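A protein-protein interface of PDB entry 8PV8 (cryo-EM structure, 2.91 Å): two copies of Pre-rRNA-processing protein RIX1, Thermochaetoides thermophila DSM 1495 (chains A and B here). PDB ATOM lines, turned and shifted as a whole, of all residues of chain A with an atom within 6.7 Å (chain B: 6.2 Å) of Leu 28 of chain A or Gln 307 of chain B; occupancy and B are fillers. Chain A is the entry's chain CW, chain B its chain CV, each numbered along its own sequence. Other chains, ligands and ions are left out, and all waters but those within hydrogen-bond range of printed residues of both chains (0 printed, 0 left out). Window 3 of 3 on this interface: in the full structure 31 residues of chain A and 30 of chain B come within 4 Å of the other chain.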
ATOM      1  N   VAL A   9       1.190  12.015  32.485  1.00  0.00           N
ATOM      2  CA  VAL A   9       2.064  11.044  31.829  1.00  0.00           C
ATOM      3  C   VAL A   9       3.039  10.440  32.835  1.00  0.00           C
ATOM      4  O   VAL A   9       3.278   9.226  32.830  1.00  0.00           O
ATOM      5  CB  VAL A   9       2.786  11.685  30.627  1.00  0.00           C
ATOM      6  CG1 VAL A   9       3.925  10.809  30.140  1.00  0.00           C
ATOM      7  CG2 VAL A   9       1.806  11.850  29.485  1.00  0.00           C
ATOM      8  N   VAL A  10       3.572  11.268  33.744  1.00  0.00           N
ATOM      9  CA  VAL A  10       4.489  10.775  34.776  1.00  0.00           C
ATOM     10  C   VAL A  10       3.809   9.731  35.654  1.00  0.00           C
ATOM     11  O   VAL A  10       4.342   8.632  35.861  1.00  0.00           O
ATOM     12  CB  VAL A  10       5.030  11.941  35.624  1.00  0.00           C
ATOM     13  CG1 VAL A  10       5.579  11.443  36.947  1.00  0.00           C
ATOM     14  CG2 VAL A  10       6.126  12.635  34.901  1.00  0.00           C
ATOM     15  N   ARG A  13       2.916   6.502  33.690  1.00  0.00           N
ATOM     16  CA  ARG A  13       4.075   5.714  33.289  1.00  0.00           C
ATOM     17  C   ARG A  13       4.738   5.051  34.488  1.00  0.00           C
ATOM     18  O   ARG A  13       5.230   3.924  34.381  1.00  0.00           O
ATOM     19  CB  ARG A  13       5.073   6.589  32.533  1.00  0.00           C
ATOM     20  CG  ARG A  13       4.806   6.649  31.039  1.00  0.00           C
ATOM     21  CD  ARG A  13       5.389   5.450  30.313  1.00  0.00           C
ATOM     22  NE  ARG A  13       5.562   5.714  28.889  1.00  0.00           N
ATOM     23  CZ  ARG A  13       6.051   4.842  28.019  1.00  0.00           C
ATOM     24  NH1 ARG A  13       6.415   3.625  28.389  1.00  0.00           N
ATOM     25  NH2 ARG A  13       6.178   5.200  26.744  1.00  0.00           N
ATOM     26  N   ARG A  24      15.654   2.487  32.225  1.00  0.00           N
ATOM     27  CA  ARG A  24      15.711   2.835  30.808  1.00  0.00           C
ATOM     28  C   ARG A  24      14.793   4.003  30.482  1.00  0.00           C
ATOM     29  O   ARG A  24      15.080   4.781  29.565  1.00  0.00           O
ATOM     30  CB  ARG A  24      15.360   1.621  29.951  1.00  0.00           C
ATOM     31  CG  ARG A  24      16.290   0.444  30.155  1.00  0.00           C
ATOM     32  CD  ARG A  24      16.126  -0.585  29.056  1.00  0.00           C
ATOM     33  NE  ARG A  24      16.763  -1.851  29.396  1.00  0.00           N
ATOM     34  CZ  ARG A  24      16.147  -2.859  29.998  1.00  0.00           C
ATOM     35  NH1 ARG A  24      14.872  -2.783  30.342  1.00  0.00           N
ATOM     36  NH2 ARG A  24      16.828  -3.971  30.262  1.00  0.00           N
ATOM     37  N   LEU A  25      13.688   4.144  31.209  1.00  0.00           N
ATOM     38  CA  LEU A  25      12.775   5.263  31.021  1.00  0.00           C
ATOM     39  C   LEU A  25      13.110   6.455  31.906  1.00  0.00           C
ATOM     40  O   LEU A  25      12.362   7.439  31.897  1.00  0.00           O
ATOM     41  CB  LEU A  25      11.323   4.832  31.273  1.00  0.00           C
ATOM     42  CG  LEU A  25      10.558   4.039  30.203  1.00  0.00           C
ATOM     43  CD1 LEU A  25      11.033   2.596  30.047  1.00  0.00           C
ATOM     44  CD2 LEU A  25       9.065   4.091  30.484  1.00  0.00           C
ATOM     45  N   CYS A  26      14.188   6.372  32.689  1.00  0.00           N
ATOM     46  CA  CYS A  26      14.643   7.526  33.466  1.00  0.00           C
ATOM     47  C   CYS A  26      14.909   8.803  32.661  1.00  0.00           C
ATOM     48  O   CYS A  26      14.565   9.882  33.175  1.00  0.00           O
ATOM     49  CB  CYS A  26      15.884   7.147  34.287  1.00  0.00           C
ATOM     50  SG  CYS A  26      15.529   6.309  35.840  1.00  0.00           S
ATOM     51  N   PRO A  27      15.532   8.787  31.463  1.00  0.00           N
ATOM     52  CA  PRO A  27      15.674  10.062  30.726  1.00  0.00           C
ATOM     53  C   PRO A  27      14.357  10.730  30.361  1.00  0.00           C
ATOM     54  O   PRO A  27      14.286  11.965  30.325  1.00  0.00           O
ATOM     55  CB  PRO A  27      16.461   9.654  29.474  1.00  0.00           C
ATOM     56  CG  PRO A  27      17.234   8.486  29.894  1.00  0.00           C
ATOM     57  CD  PRO A  27      16.333   7.729  30.812  1.00  0.00           C
ATOM     58  N   LEU A  28      13.310   9.951  30.088  1.00  0.00           N
ATOM     59  CA  LEU A  28      12.011  10.536  29.769  1.00  0.00           C
ATOM     60  C   LEU A  28      11.353  11.119  31.012  1.00  0.00           C
ATOM     61  O   LEU A  28      10.819  12.240  30.983  1.00  0.00           O
ATOM     62  CB  LEU A  28      11.112   9.472  29.143  1.00  0.00           C
ATOM     63  CG  LEU A  28      11.726   8.628  28.026  1.00  0.00           C
ATOM     64  CD1 LEU A  28      10.672   7.730  27.423  1.00  0.00           C
ATOM     65  CD2 LEU A  28      12.337   9.517  26.948  1.00  0.00           C
ATOM     66  N   LEU A  29      11.389  10.365  32.115  1.00  0.00           N
ATOM     67  CA  LEU A  29      10.754  10.798  33.352  1.00  0.00           C
ATOM     68  C   LEU A  29      11.420  12.046  33.909  1.00  0.00           C
ATOM     69  O   LEU A  29      10.742  12.925  34.451  1.00  0.00           O
ATOM     70  CB  LEU A  29      10.791   9.664  34.376  1.00  0.00           C
ATOM     71  CG  LEU A  29       9.995   8.413  34.002  1.00  0.00           C
ATOM     72  CD1 LEU A  29      10.428   7.232  34.852  1.00  0.00           C
ATOM     73  CD2 LEU A  29       8.503   8.666  34.150  1.00  0.00           C
ATOM     74  N   ILE A  30      12.746  12.146  33.773  1.00  0.00           N
ATOM     75  CA  ILE A  30      13.459  13.326  34.257  1.00  0.00           C
ATOM     76  C   ILE A  30      13.019  14.570  33.495  1.00  0.00           C
ATOM     77  O   ILE A  30      12.707  15.600  34.101  1.00  0.00           O
ATOM     78  CB  ILE A  30      14.981  13.105  34.173  1.00  0.00           C
ATOM     79  CG1 ILE A  30      15.447  12.195  35.312  1.00  0.00           C
ATOM     80  CG2 ILE A  30      15.735  14.429  34.205  1.00  0.00           C
ATOM     81  CD1 ILE A  30      16.952  12.080  35.434  1.00  0.00           C
ATOM     82  N   ASN A  31      12.953  14.484  32.162  1.00  0.00           N
ATOM     83  CA  ASN A  31      12.518  15.627  31.362  1.00  0.00           C
ATOM     84  C   ASN A  31      11.078  16.007  31.677  1.00  0.00           C
ATOM     85  O   ASN A  31      10.737  17.196  31.736  1.00  0.00           O
ATOM     86  CB  ASN A  31      12.674  15.323  29.872  1.00  0.00           C
ATOM     87  CG  ASN A  31      14.095  14.959  29.496  1.00  0.00           C
ATOM     88  OD1 ASN A  31      15.055  15.436  30.102  1.00  0.00           O
ATOM     89  ND2 ASN A  31      14.237  14.104  28.490  1.00  0.00           N
ATOM     90  N   HIS A  32      10.224  15.010  31.915  1.00  0.00           N
ATOM     91  CA  HIS A  32       8.841  15.306  32.274  1.00  0.00           C
ATOM     92  C   HIS A  32       8.741  15.991  33.637  1.00  0.00           C
ATOM     93  O   HIS A  32       7.932  16.908  33.816  1.00  0.00           O
ATOM     94  CB  HIS A  32       8.015  14.027  32.234  1.00  0.00           C
ATOM     95  CG  HIS A  32       7.675  13.572  30.851  1.00  0.00           C
ATOM     96  ND1 HIS A  32       8.297  12.503  30.243  1.00  0.00           N
ATOM     97  CD2 HIS A  32       6.775  14.042  29.954  1.00  0.00           C
ATOM     98  CE1 HIS A  32       7.797  12.334  29.033  1.00  0.00           C
ATOM     99  NE2 HIS A  32       6.872  13.255  28.832  1.00  0.00           N
ATOM    100  N   VAL A  33       9.566  15.581  34.606  1.00  0.00           N
ATOM    101  CA  VAL A  33       9.532  16.231  35.919  1.00  0.00           C
ATOM    102  C   VAL A  33      10.075  17.657  35.832  1.00  0.00           C
ATOM    103  O   VAL A  33       9.536  18.579  36.460  1.00  0.00           O
ATOM    104  CB  VAL A  33      10.283  15.385  36.966  1.00  0.00           C
ATOM    105  CG1 VAL A  33      10.358  16.113  38.294  1.00  0.00           C
ATOM    106  CG2 VAL A  33       9.568  14.071  37.180  1.00  0.00           C
ATOM    107  N   THR B 212      14.586   3.349  19.877  1.00  0.00           N
ATOM    108  CA  THR B 212      13.343   3.693  20.546  1.00  0.00           C
ATOM    109  C   THR B 212      13.358   3.103  21.950  1.00  0.00           C
ATOM    110  O   THR B 212      14.289   2.395  22.342  1.00  0.00           O
ATOM    111  CB  THR B 212      12.129   3.187  19.756  1.00  0.00           C
ATOM    112  OG1 THR B 212      12.257   1.778  19.532  1.00  0.00           O
ATOM    113  CG2 THR B 212      12.042   3.892  18.416  1.00  0.00           C
ATOM    114  N   SER B 213      12.310   3.400  22.712  1.00  0.00           N
ATOM    115  CA  SER B 213      12.152   2.872  24.058  1.00  0.00           C
ATOM    116  C   SER B 213      11.556   1.472  24.071  1.00  0.00           C
ATOM    117  O   SER B 213      11.414   0.880  25.145  1.00  0.00           O
ATOM    118  CB  SER B 213      11.285   3.815  24.897  1.00  0.00           C
ATOM    119  OG  SER B 213      10.003   3.978  24.315  1.00  0.00           O
ATOM    120  N   PRO B 290      -0.231   3.374  18.456  1.00  0.00           N
ATOM    121  CA  PRO B 290       0.488   3.487  17.183  1.00  0.00           C
ATOM    122  C   PRO B 290       1.707   2.579  17.151  1.00  0.00           C
ATOM    123  O   PRO B 290       2.329   2.295  18.176  1.00  0.00           O
ATOM    124  CB  PRO B 290       0.890   4.966  17.126  1.00  0.00           C
ATOM    125  CG  PRO B 290       0.843   5.433  18.534  1.00  0.00           C
ATOM    126  CD  PRO B 290      -0.248   4.651  19.192  1.00  0.00           C
ATOM    127  N   GLY B 305       4.051   2.202  20.282  1.00  0.00           N
ATOM    128  CA  GLY B 305       3.831   3.200  21.306  1.00  0.00           C
ATOM    129  C   GLY B 305       4.085   4.600  20.795  1.00  0.00           C
ATOM    130  O   GLY B 305       4.957   4.811  19.945  1.00  0.00           O
ATOM    131  N   LEU B 306       3.323   5.567  21.310  1.00  0.00           N
ATOM    132  CA  LEU B 306       3.435   6.940  20.831  1.00  0.00           C
ATOM    133  C   LEU B 306       4.777   7.559  21.200  1.00  0.00           C
ATOM    134  O   LEU B 306       5.373   8.288  20.397  1.00  0.00           O
ATOM    135  CB  LEU B 306       2.291   7.776  21.391  1.00  0.00           C
ATOM    136  CG  LEU B 306       2.247   9.213  20.888  1.00  0.00           C
ATOM    137  CD1 LEU B 306       2.042   9.233  19.396  1.00  0.00           C
ATOM    138  CD2 LEU B 306       1.135   9.932  21.571  1.00  0.00           C
ATOM    139  N   GLN B 307       5.271   7.278  22.408  1.00  0.00           N
ATOM    140  CA  GLN B 307       6.567   7.807  22.818  1.00  0.00           C
ATOM    141  C   GLN B 307       7.691   7.180  22.004  1.00  0.00           C
ATOM    142  O   GLN B 307       8.663   7.854  21.640  1.00  0.00           O
ATOM    143  CB  GLN B 307       6.780   7.570  24.313  1.00  0.00           C
ATOM    144  CG  GLN B 307       8.109   8.072  24.840  1.00  0.00           C
ATOM    145  CD  GLN B 307       8.138   9.579  25.029  1.00  0.00           C
ATOM    146  OE1 GLN B 307       7.113  10.253  24.922  1.00  0.00           O
ATOM    147  NE2 GLN B 307       9.320  10.115  25.308  1.00  0.00           N
ATOM    148  N   ALA B 308       7.563   5.886  21.696  1.00  0.00           N
ATOM    149  CA  ALA B 308       8.526   5.230  20.820  1.00  0.00           C
ATOM    150  C   ALA B 308       8.509   5.829  19.421  1.00  0.00           C
ATOM    151  O   ALA B 308       9.567   6.003  18.809  1.00  0.00           O
ATOM    152  CB  ALA B 308       8.247   3.729  20.761  1.00  0.00           C
ATOM    153  N   GLY B 309       7.324   6.162  18.905  1.00  0.00           N
ATOM    154  CA  GLY B 309       7.254   6.820  17.610  1.00  0.00           C
ATOM    155  C   GLY B 309       7.854   8.213  17.622  1.00  0.00           C
ATOM    156  O   GLY B 309       8.496   8.629  16.654  1.00  0.00           O
ATOM    157  N   ALA B 310       7.651   8.950  18.717  1.00  0.00           N
ATOM    158  CA  ALA B 310       8.275  10.263  18.859  1.00  0.00           C
ATOM    159  C   ALA B 310       9.794  10.152  18.902  1.00  0.00           C
ATOM    160  O   ALA B 310      10.499  10.960  18.284  1.00  0.00           O
ATOM    161  CB  ALA B 310       7.755  10.959  20.115  1.00  0.00           C
ATOM    162  N   GLU B 311      10.314   9.150  19.618  1.00  0.00           N
ATOM    163  CA  GLU B 311      11.757   8.928  19.658  1.00  0.00           C
ATOM    164  C   GLU B 311      12.295   8.522  18.292  1.00  0.00           C
ATOM    165  O   GLU B 311      13.387   8.946  17.898  1.00  0.00           O
ATOM    166  CB  GLU B 311      12.097   7.867  20.704  1.00  0.00           C
ATOM    167  CG  GLU B 311      11.875   8.314  22.137  1.00  0.00           C
ATOM    168  CD  GLU B 311      12.153   7.212  23.137  1.00  0.00           C
ATOM    169  OE1 GLU B 311      12.471   6.085  22.707  1.00  0.00           O
ATOM    170  OE2 GLU B 311      12.055   7.471  24.353  1.00  0.00           O
ATOM    171  N   ARG B 312      11.539   7.701  17.556  1.00  0.00           N
ATOM    172  CA  ARG B 312      11.932   7.312  16.203  1.00  0.00           C
ATOM    173  C   ARG B 312      11.989   8.520  15.275  1.00  0.00           C
ATOM    174  O   ARG B 312      12.933   8.671  14.490  1.00  0.00           O
ATOM    175  CB  ARG B 312      10.953   6.273  15.659  1.00  0.00           C
ATOM    176  CG  ARG B 312      11.225   5.850  14.228  1.00  0.00           C
ATOM    177  CD  ARG B 312      12.366   4.861  14.168  1.00  0.00           C
ATOM    178  NE  ARG B 312      12.042   3.641  14.894  1.00  0.00           N
ATOM    179  CZ  ARG B 312      12.914   2.690  15.193  1.00  0.00           C
ATOM    180  NH1 ARG B 312      14.189   2.792  14.858  1.00  0.00           N
ATOM    181  NH2 ARG B 312      12.501   1.616  15.860  1.00  0.00           N
ATOM    182  N   GLU B 373      -0.111  12.481  25.738  1.00  0.00           N
ATOM    183  CA  GLU B 373       1.233  12.022  25.458  1.00  0.00           C
ATOM    184  C   GLU B 373       1.791  12.652  24.194  1.00  0.00           C
ATOM    185  O   GLU B 373       2.978  12.989  24.163  1.00  0.00           O
ATOM    186  CB  GLU B 373       1.264  10.490  25.345  1.00  0.00           C
ATOM    187  CG  GLU B 373       2.650   9.879  25.231  1.00  0.00           C
ATOM    188  CD  GLU B 373       2.615   8.365  25.327  1.00  0.00           C
ATOM    189  OE1 GLU B 373       1.502   7.805  25.418  1.00  0.00           O
ATOM    190  OE2 GLU B 373       3.694   7.739  25.323  1.00  0.00           O
ATOM    191  N   SER B 376       2.910  16.232  24.963  1.00  0.00           N
ATOM    192  CA  SER B 376       4.245  16.226  25.543  1.00  0.00           C
ATOM    193  C   SER B 376       5.321  15.768  24.572  1.00  0.00           C
ATOM    194  O   SER B 376       6.493  16.080  24.779  1.00  0.00           O
ATOM    195  CB  SER B 376       4.283  15.328  26.786  1.00  0.00           C
ATOM    196  OG  SER B 376       3.835  14.018  26.485  1.00  0.00           O
ATOM    197  N   ALA B 377       4.951  15.021  23.530  1.00  0.00           N
ATOM    198  CA  ALA B 377       5.945  14.512  22.591  1.00  0.00           C
ATOM    199  C   ALA B 377       6.397  15.577  21.595  1.00  0.00           C
ATOM    200  O   ALA B 377       7.534  15.528  21.111  1.00  0.00           O
ATOM    201  CB  ALA B 377       5.391  13.293  21.858  1.00  0.00           C
ATOM    202  N   ASP B 380      10.179  17.883  21.828  1.00  0.00           N
ATOM    203  CA  ASP B 380      11.446  17.274  21.429  1.00  0.00           C
ATOM    204  C   ASP B 380      11.570  17.194  19.910  1.00  0.00           C
ATOM    205  O   ASP B 380      12.650  17.426  19.351  1.00  0.00           O
ATOM    206  CB  ASP B 380      11.579  15.886  22.054  1.00  0.00           C
ATOM    207  CG  ASP B 380      11.740  15.941  23.559  1.00  0.00           C
ATOM    208  OD1 ASP B 380      12.290  16.944  24.060  1.00  0.00           O
ATOM    209  OD2 ASP B 380      11.312  14.987  24.241  1.00  0.00           O
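The backbone carbonyl oxygen (O) of Leu 28 of chain A lies within hydrogen-bond range of a ring nitrogen (ND1) of His 32 of chain A, 2.6 Å away. The backbone NH (N) of Ser 213 of chain B is in hydrogen-bond range of the side-chain carboxylate (OE1) of Glu 311 of chain B (2.7 Å). N of Gln 307 of chain B sits close to OE2 of Glu 373 of chain B (3.3 Å). The side-chain hydroxyl (OG) of Ser 376 of chain B is in hydrogen-bond range of the backbone carbonyl oxygen (O) of Glu 373 of chain B.
Of the 15 printed residues of chain B, 4 touch a printed residue of chain A. Printed residues of chain B that touch a printed residue of chain A: Gln 307, Glu 311, Glu 373 and Ser 376. Among the printed residues, Asp or Glu carboxylates within 4 Å of a Lys or Arg side-chain nitrogen of the other chain: Arg 13 of chain A with Glu 373 of chain B.
No position is printed for both chains. Of the 5 pairs that touch across the chains among the printed residues, none has its exchanged pair printed and touching as well.
OE2 of Glu 373 of chain B lies within salt-bridge range of NH2 of Arg 13 of chain A, 3.8 Å away.
Among the printed residues, merely in contact across the chains: Leu 28 of chain A with Glu 311 of chain B, Arg 13 of chain A with Gln 307 of chain B, Leu 28 of chain A with Gln 307 of chain B and His 32 of chain A with Ser 376 of chain B.
Of chain B, only Gln 307 (3.5 Å) and Glu 311 (3.3 Å) come within 4 Å of Leu 28 of chain A. Gln 307 of chain B touches two residues of chain A. Printed residues of chain A within 4 Å of Glu 373 of chain B: Arg 13. Of the printed residues of chain B, His 32 of chain A touches Ser 376 (3.9 Å). Of the printed residues of chain A, Glu 311 of chain B touches Leu 28 (3.3 Å). Printed residues of chain A within 4 Å of Ser 376 of chain B: His 32. Asp 380 of chain B touches none of the printed residues of chain A. Arg 24 of chain A touches none of the printed residues of chain B.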
